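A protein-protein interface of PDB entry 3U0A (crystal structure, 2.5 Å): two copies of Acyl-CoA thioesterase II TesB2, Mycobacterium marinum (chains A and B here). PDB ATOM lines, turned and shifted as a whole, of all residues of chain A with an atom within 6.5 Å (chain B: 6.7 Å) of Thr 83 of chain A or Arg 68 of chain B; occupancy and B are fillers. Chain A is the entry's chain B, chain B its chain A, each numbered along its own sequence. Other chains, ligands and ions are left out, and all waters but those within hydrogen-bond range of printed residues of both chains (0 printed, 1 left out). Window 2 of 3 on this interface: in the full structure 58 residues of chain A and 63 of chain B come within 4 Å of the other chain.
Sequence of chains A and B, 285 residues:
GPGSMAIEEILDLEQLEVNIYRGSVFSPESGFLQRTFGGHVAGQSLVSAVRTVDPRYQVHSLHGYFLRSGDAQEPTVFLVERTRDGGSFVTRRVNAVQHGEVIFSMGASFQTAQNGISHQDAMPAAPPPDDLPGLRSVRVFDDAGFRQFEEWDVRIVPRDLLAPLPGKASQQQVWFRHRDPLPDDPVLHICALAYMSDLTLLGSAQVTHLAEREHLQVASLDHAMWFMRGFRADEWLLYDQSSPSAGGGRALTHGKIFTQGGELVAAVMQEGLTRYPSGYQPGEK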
ATOM      1  N   GLU A  81      19.941  30.843   8.261  1.00  0.00           N
ATOM      2  CA  GLU A  81      19.534  30.068   9.430  1.00  0.00           C
ATOM      3  C   GLU A  81      20.259  30.558  10.693  1.00  0.00           C
ATOM      4  O   GLU A  81      21.474  30.721  10.696  1.00  0.00           O
ATOM      5  CB  GLU A  81      19.838  28.588   9.188  1.00  0.00           C
ATOM      6  CG  GLU A  81      19.630  27.667  10.394  1.00  0.00           C
ATOM      7  CD  GLU A  81      20.231  26.279  10.160  1.00  0.00           C
ATOM      8  OE1 GLU A  81      19.743  25.556   9.240  1.00  0.00           O
ATOM      9  OE2 GLU A  81      21.221  25.927  10.876  1.00  0.00           O
ATOM     10  N   ARG A  82      19.496  30.774  11.765  1.00  0.00           N
ATOM     11  CA  ARG A  82      20.054  31.230  13.044  1.00  0.00           C
ATOM     12  C   ARG A  82      20.348  30.049  13.943  1.00  0.00           C
ATOM     13  O   ARG A  82      19.619  29.757  14.857  1.00  0.00           O
ATOM     14  CB  ARG A  82      19.115  32.223  13.708  1.00  0.00           C
ATOM     15  CG  ARG A  82      18.916  33.425  12.831  1.00  0.00           C
ATOM     16  CD  ARG A  82      18.303  34.610  13.572  1.00  0.00           C
ATOM     17  NE  ARG A  82      17.993  35.701  12.648  1.00  0.00           N
ATOM     18  CZ  ARG A  82      17.717  36.946  13.008  1.00  0.00           C
ATOM     19  NH1 ARG A  82      17.690  37.287  14.291  1.00  0.00           N
ATOM     20  NH2 ARG A  82      17.457  37.855  12.061  1.00  0.00           N
ATOM     21  N   THR A  83      21.460  29.409  13.648  1.00  0.00           N
ATOM     22  CA  THR A  83      21.865  28.150  14.212  1.00  0.00           C
ATOM     23  C   THR A  83      21.943  28.177  15.759  1.00  0.00           C
ATOM     24  O   THR A  83      21.341  27.351  16.384  1.00  0.00           O
ATOM     25  CB  THR A  83      23.211  27.721  13.557  1.00  0.00           C
ATOM     26  OG1 THR A  83      23.088  27.793  12.135  1.00  0.00           O
ATOM     27  CG2 THR A  83      23.581  26.323  13.908  1.00  0.00           C
ATOM     28  N   ARG A  84      22.686  29.111  16.355  1.00  0.00           N
ATOM     29  CA  ARG A  84      22.603  29.392  17.796  1.00  0.00           C
ATOM     30  C   ARG A  84      22.777  30.885  18.043  1.00  0.00           C
ATOM     31  O   ARG A  84      23.350  31.606  17.219  1.00  0.00           O
ATOM     32  CB  ARG A  84      23.659  28.607  18.677  1.00  0.00           C
ATOM     33  CG  ARG A  84      25.118  29.031  18.447  1.00  0.00           C
ATOM     34  CD  ARG A  84      26.074  29.005  19.662  1.00  0.00           C
ATOM     35  NE  ARG A  84      27.494  28.929  19.201  1.00  0.00           N
ATOM     36  CZ  ARG A  84      28.520  28.466  19.925  1.00  0.00           C
ATOM     37  NH1 ARG A  84      28.327  28.117  21.198  1.00  0.00           N
ATOM     38  NH2 ARG A  84      29.757  28.374  19.390  1.00  0.00           N
ATOM     39  N   ASP A  85      22.327  31.317  19.218  1.00  0.00           N
ATOM     40  CA  ASP A  85      22.656  32.635  19.731  1.00  0.00           C
ATOM     41  C   ASP A  85      22.969  32.429  21.202  1.00  0.00           C
ATOM     42  O   ASP A  85      22.046  32.172  22.005  1.00  0.00           O
ATOM     43  CB  ASP A  85      21.456  33.600  19.567  1.00  0.00           C
ATOM     44  CG  ASP A  85      21.164  33.962  18.100  1.00  0.00           C
ATOM     45  OD1 ASP A  85      20.704  33.091  17.334  1.00  0.00           O
ATOM     46  OD2 ASP A  85      21.403  35.114  17.724  1.00  0.00           O
ATOM     47  N   THR A  91      26.106  31.729  15.751  1.00  0.00           N
ATOM     48  CA  THR A  91      26.478  30.898  14.605  1.00  0.00           C
ATOM     49  C   THR A  91      25.383  30.944  13.561  1.00  0.00           C
ATOM     50  O   THR A  91      24.203  30.830  13.897  1.00  0.00           O
ATOM     51  CB  THR A  91      26.736  29.425  15.017  1.00  0.00           C
ATOM     52  OG1 THR A  91      27.581  29.365  16.162  1.00  0.00           O
ATOM     53  CG2 THR A  91      27.405  28.624  13.876  1.00  0.00           C
ATOM     54  N   ARG A  92      25.774  31.090  12.297  1.00  0.00           N
ATOM     55  CA  ARG A  92      24.828  31.146  11.184  1.00  0.00           C
ATOM     56  C   ARG A  92      25.165  30.205  10.036  1.00  0.00           C
ATOM     57  O   ARG A  92      26.323  29.924   9.789  1.00  0.00           O
ATOM     58  CB  ARG A  92      24.781  32.557  10.636  1.00  0.00           C
ATOM     59  CG  ARG A  92      24.338  33.568  11.642  1.00  0.00           C
ATOM     60  CD  ARG A  92      22.888  33.356  11.992  1.00  0.00           C
ATOM     61  NE  ARG A  92      22.362  34.441  12.806  1.00  0.00           N
ATOM     62  CZ  ARG A  92      22.145  34.366  14.124  1.00  0.00           C
ATOM     63  NH1 ARG A  92      22.420  33.266  14.812  1.00  0.00           N
ATOM     64  NH2 ARG A  92      21.616  35.391  14.751  1.00  0.00           N
ATOM     65  N   ARG A  93      24.145  29.737   9.322  1.00  0.00           N
ATOM     66  CA  ARG A  93      24.366  29.021   8.084  1.00  0.00           C
ATOM     67  C   ARG A  93      23.633  29.760   6.983  1.00  0.00           C
ATOM     68  O   ARG A  93      22.603  30.335   7.205  1.00  0.00           O
ATOM     69  CB  ARG A  93      23.960  27.535   8.152  1.00  0.00           C
ATOM     70  CG  ARG A  93      24.667  26.705   9.224  1.00  0.00           C
ATOM     71  CD  ARG A  93      24.553  25.171   9.035  1.00  0.00           C
ATOM     72  NE  ARG A  93      23.252  24.562   9.436  1.00  0.00           N
ATOM     73  CZ  ARG A  93      22.819  23.331   9.071  1.00  0.00           C
ATOM     74  NH1 ARG A  93      23.569  22.527   8.315  1.00  0.00           N
ATOM     75  NH2 ARG A  93      21.611  22.909   9.436  1.00  0.00           N
ATOM     76  N   GLN B  34      35.863  16.748  27.983  1.00  0.00           N
ATOM     77  CA  GLN B  34      34.855  17.270  27.016  1.00  0.00           C
ATOM     78  C   GLN B  34      35.374  17.178  25.567  1.00  0.00           C
ATOM     79  O   GLN B  34      34.596  16.968  24.610  1.00  0.00           O
ATOM     80  CB  GLN B  34      34.423  18.720  27.414  1.00  0.00           C
ATOM     81  CG  GLN B  34      33.656  19.556  26.368  1.00  0.00           C
ATOM     82  CD  GLN B  34      32.296  18.984  25.979  1.00  0.00           C
ATOM     83  OE1 GLN B  34      32.124  18.430  24.879  1.00  0.00           O
ATOM     84  NE2 GLN B  34      31.315  19.125  26.879  1.00  0.00           N
ATOM     85  N   PHE B  37      34.392  13.689  24.202  1.00  0.00           N
ATOM     86  CA  PHE B  37      33.028  13.627  23.742  1.00  0.00           C
ATOM     87  C   PHE B  37      32.871  14.372  22.407  1.00  0.00           C
ATOM     88  O   PHE B  37      32.287  13.850  21.480  1.00  0.00           O
ATOM     89  CB  PHE B  37      32.065  14.169  24.798  1.00  0.00           C
ATOM     90  CG  PHE B  37      30.625  13.953  24.457  1.00  0.00           C
ATOM     91  CD1 PHE B  37      30.123  12.682  24.252  1.00  0.00           C
ATOM     92  CD2 PHE B  37      29.763  15.017  24.304  1.00  0.00           C
ATOM     93  CE1 PHE B  37      28.763  12.477  23.930  1.00  0.00           C
ATOM     94  CE2 PHE B  37      28.416  14.821  24.003  1.00  0.00           C
ATOM     95  CZ  PHE B  37      27.911  13.554  23.819  1.00  0.00           C
ATOM     96  N   TYR B  65      31.373  22.800  13.176  1.00  0.00           N
ATOM     97  CA  TYR B  65      31.331  23.750  14.243  1.00  0.00           C
ATOM     98  C   TYR B  65      30.833  23.070  15.540  1.00  0.00           C
ATOM     99  O   TYR B  65      29.747  22.498  15.581  1.00  0.00           O
ATOM    100  CB  TYR B  65      30.376  24.868  13.851  1.00  0.00           C
ATOM    101  CG  TYR B  65      30.973  26.048  13.108  1.00  0.00           C
ATOM    102  CD1 TYR B  65      32.121  26.689  13.575  1.00  0.00           C
ATOM    103  CD2 TYR B  65      30.339  26.575  11.978  1.00  0.00           C
ATOM    104  CE1 TYR B  65      32.653  27.786  12.914  1.00  0.00           C
ATOM    105  CE2 TYR B  65      30.849  27.678  11.314  1.00  0.00           C
ATOM    106  CZ  TYR B  65      32.015  28.297  11.780  1.00  0.00           C
ATOM    107  OH  TYR B  65      32.548  29.398  11.102  1.00  0.00           O
ATOM    108  N   PHE B  66      31.635  23.159  16.600  1.00  0.00           N
ATOM    109  CA  PHE B  66      31.259  22.628  17.907  1.00  0.00           C
ATOM    110  C   PHE B  66      30.380  23.648  18.612  1.00  0.00           C
ATOM    111  O   PHE B  66      30.847  24.677  19.094  1.00  0.00           O
ATOM    112  CB  PHE B  66      32.496  22.350  18.733  1.00  0.00           C
ATOM    113  CG  PHE B  66      33.366  21.272  18.170  1.00  0.00           C
ATOM    114  CD1 PHE B  66      33.117  19.941  18.483  1.00  0.00           C
ATOM    115  CD2 PHE B  66      34.412  21.579  17.338  1.00  0.00           C
ATOM    116  CE1 PHE B  66      33.897  18.935  18.002  1.00  0.00           C
ATOM    117  CE2 PHE B  66      35.201  20.573  16.839  1.00  0.00           C
ATOM    118  CZ  PHE B  66      34.950  19.245  17.183  1.00  0.00           C
ATOM    119  N   LEU B  67      29.088  23.377  18.622  1.00  0.00           N
ATOM    120  CA  LEU B  67      28.148  24.374  19.056  1.00  0.00           C
ATOM    121  C   LEU B  67      27.946  24.302  20.570  1.00  0.00           C
ATOM    122  O   LEU B  67      27.953  25.317  21.236  1.00  0.00           O
ATOM    123  CB  LEU B  67      26.831  24.235  18.280  1.00  0.00           C
ATOM    124  CG  LEU B  67      26.867  24.404  16.751  1.00  0.00           C
ATOM    125  CD1 LEU B  67      25.473  24.294  16.206  1.00  0.00           C
ATOM    126  CD2 LEU B  67      27.483  25.714  16.335  1.00  0.00           C
ATOM    127  N   ARG B  68      27.786  23.099  21.102  1.00  0.00           N
ATOM    128  CA  ARG B  68      27.409  22.920  22.502  1.00  0.00           C
ATOM    129  C   ARG B  68      28.076  21.735  23.119  1.00  0.00           C
ATOM    130  O   ARG B  68      28.499  20.824  22.434  1.00  0.00           O
ATOM    131  CB  ARG B  68      25.905  22.700  22.622  1.00  0.00           C
ATOM    132  CG  ARG B  68      25.131  23.971  22.892  1.00  0.00           C
ATOM    133  CD  ARG B  68      23.664  23.756  22.576  1.00  0.00           C
ATOM    134  NE  ARG B  68      23.352  24.018  21.157  1.00  0.00           N
ATOM    135  CZ  ARG B  68      22.610  25.035  20.724  1.00  0.00           C
ATOM    136  NH1 ARG B  68      22.387  25.192  19.397  1.00  0.00           N
ATOM    137  NH2 ARG B  68      22.087  25.891  21.607  1.00  0.00           N
ATOM    138  N   SER B  69      28.117  21.737  24.441  1.00  0.00           N
ATOM    139  CA  SER B  69      28.777  20.682  25.227  1.00  0.00           C
ATOM    140  C   SER B  69      28.111  19.261  25.120  1.00  0.00           C
ATOM    141  O   SER B  69      28.785  18.223  25.000  1.00  0.00           O
ATOM    142  CB  SER B  69      28.779  21.144  26.677  1.00  0.00           C
ATOM    143  OG  SER B  69      27.509  21.728  26.958  1.00  0.00           O
ATOM    144  N   GLY B  70      26.791  19.231  25.172  1.00  0.00           N
ATOM    145  CA  GLY B  70      26.093  17.955  25.209  1.00  0.00           C
ATOM    146  C   GLY B  70      26.168  17.286  26.572  1.00  0.00           C
ATOM    147  O   GLY B  70      26.631  17.879  27.535  1.00  0.00           O
ATOM    148  N   ASN B  95      23.648  17.399  11.263  1.00  0.00           N
ATOM    149  CA  ASN B  95      23.432  17.995  12.575  1.00  0.00           C
ATOM    150  C   ASN B  95      23.345  16.911  13.655  1.00  0.00           C
ATOM    151  O   ASN B  95      22.501  16.056  13.594  1.00  0.00           O
ATOM    152  CB  ASN B  95      22.139  18.813  12.608  1.00  0.00           C
ATOM    153  CG  ASN B  95      22.268  20.188  11.971  1.00  0.00           C
ATOM    154  OD1 ASN B  95      23.375  20.687  11.666  1.00  0.00           O
ATOM    155  ND2 ASN B  95      21.117  20.827  11.782  1.00  0.00           N
ATOM    156  N   GLU B 101      18.447  20.051  20.649  1.00  0.00           N
ATOM    157  CA  GLU B 101      19.451  21.090  20.391  1.00  0.00           C
ATOM    158  C   GLU B 101      20.529  20.575  19.443  1.00  0.00           C
ATOM    159  O   GLU B 101      21.011  19.459  19.610  1.00  0.00           O
ATOM    160  CB  GLU B 101      20.111  21.554  21.699  1.00  0.00           C
ATOM    161  CG  GLU B 101      19.165  22.017  22.826  1.00  0.00           C
ATOM    162  CD  GLU B 101      18.515  23.397  22.594  1.00  0.00           C
ATOM    163  OE1 GLU B 101      18.275  23.807  21.407  1.00  0.00           O
ATOM    164  OE2 GLU B 101      18.220  24.097  23.609  1.00  0.00           O
ATOM    165  N   VAL B 102      20.918  21.381  18.454  1.00  0.00           N
ATOM    166  CA  VAL B 102      22.083  21.026  17.631  1.00  0.00           C
ATOM    167  C   VAL B 102      23.379  21.306  18.444  1.00  0.00           C
ATOM    168  O   VAL B 102      23.643  22.441  18.848  1.00  0.00           O
ATOM    169  CB  VAL B 102      22.096  21.750  16.258  1.00  0.00           C
ATOM    170  CG1 VAL B 102      23.345  21.359  15.465  1.00  0.00           C
ATOM    171  CG2 VAL B 102      20.845  21.425  15.480  1.00  0.00           C
ATOM    172  N   ILE B 103      24.130  20.237  18.721  1.00  0.00           N
ATOM    173  CA  ILE B 103      25.363  20.304  19.516  1.00  0.00           C
ATOM    174  C   ILE B 103      26.614  20.418  18.640  1.00  0.00           C
ATOM    175  O   ILE B 103      27.614  20.955  19.053  1.00  0.00           O
ATOM    176  CB  ILE B 103      25.482  19.102  20.495  1.00  0.00           C
ATOM    177  CG1 ILE B 103      25.797  17.778  19.773  1.00  0.00           C
ATOM    178  CG2 ILE B 103      24.213  18.943  21.340  1.00  0.00           C
ATOM    179  CD1 ILE B 103      25.981  16.621  20.752  1.00  0.00           C
ATOM    180  N   PHE B 104      26.514  19.916  17.415  1.00  0.00           N
ATOM    181  CA  PHE B 104      27.591  19.907  16.457  1.00  0.00           C
ATOM    182  C   PHE B 104      27.001  19.971  15.070  1.00  0.00           C
ATOM    183  O   PHE B 104      26.052  19.303  14.785  1.00  0.00           O
ATOM    184  CB  PHE B 104      28.448  18.626  16.622  1.00  0.00           C
ATOM    185  CG  PHE B 104      29.613  18.548  15.672  1.00  0.00           C
ATOM    186  CD1 PHE B 104      30.745  19.330  15.865  1.00  0.00           C
ATOM    187  CD2 PHE B 104      29.562  17.740  14.549  1.00  0.00           C
ATOM    188  CE1 PHE B 104      31.800  19.281  14.968  1.00  0.00           C
ATOM    189  CE2 PHE B 104      30.613  17.680  13.669  1.00  0.00           C
ATOM    190  CZ  PHE B 104      31.732  18.448  13.874  1.00  0.00           C
ATOM    191  N   SER B 105      27.580  20.769  14.204  1.00  0.00           N
ATOM    192  CA  SER B 105      27.100  20.910  12.823  1.00  0.00           C
ATOM    193  C   SER B 105      28.276  20.858  11.855  1.00  0.00           C
ATOM    194  O   SER B 105      29.322  21.425  12.091  1.00  0.00           O
ATOM    195  CB  SER B 105      26.320  22.214  12.620  1.00  0.00           C
ATOM    196  OG  SER B 105      25.655  22.219  11.362  1.00  0.00           O
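No position is printed for both chains.
Of the 8 printed residues of chain A, 4 touch a printed residue of chain B. Of the 14 printed residues of chain B, 5 touch a printed residue of chain A.
Among the printed residues, merely in contact across the chains: Thr 83 of chain A with Leu 67 of chain B, Thr 91 of chain A with Leu 67 of chain B, Arg 93 of chain A with Ser 105 of chain B, Arg 84 of chain A with Arg 68 of chain B, Thr 83 of chain A with Arg 68 of chain B and Arg 84 of chain A with Phe 66 of chain B.
Thr 83 of chain A touches just these residues of chain B: Leu 67 (3.6 Å) and Arg 68 (3.9 Å). Of chain A, only Thr 83 and Arg 84 come within 4 Å of Arg 68 of chain B. Printed residues of chain A within 4 Å of Leu 67 of chain B: Thr 83, Arg 84 and Thr 91. Printed residues of chain A within 4 Å of Phe 66 of chain B: Arg 84. Of the printed residues of chain B, Arg 93 of chain A touches Asn 95 (3.2 Å) and Ser 105 (3.7 Å). Of the printed residues of chain A, Asn 95 of chain B touches Arg 93. Of the printed residues of chain B, Arg 84 of chain A touches Phe 66, Leu 67 and Arg 68.
The backbone NH of Leu 67 of chain B sits at hydrogen-bond distance from the backbone carbonyl oxygen of Ile 103 of chain B, at 2.9 Å. The backbone carbonyl oxygen (O) of Val 102 of chain B is in hydrogen-bond range of the guanidinium group (NE) of Arg 68 of chain B (2.8 Å). O of Ile 103 of chain B is in hydrogen-bond range of N of Arg 68 of chain B (3.0 Å). OE2 of Glu 81 of chain A is in salt-bridge range of NE of Arg 93 of chain A. The guanidinium group (NE) of Arg 84 of chain A lies within hydrogen-bond range of the side-chain hydroxyl (OG1) of Thr 91 of chain A (3.1 Å). The backbone carbonyl oxygen of Arg 84 of chain A is in hydrogen-bond range of the guanidinium group of Arg 92 of chain A, 3.1 Å away.
The backbone carbonyl oxygen (O) of Leu 67 of chain B sits at hydrogen-bond distance from the guanidinium group (NH1) of Arg 84 of chain A, at 2.8 Å. The guanidinium group (NH2) of Arg 93 of chain A sits close to the side-chain amide nitrogen (ND2) of Asn 95 of chain B, 3.2 Å away.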
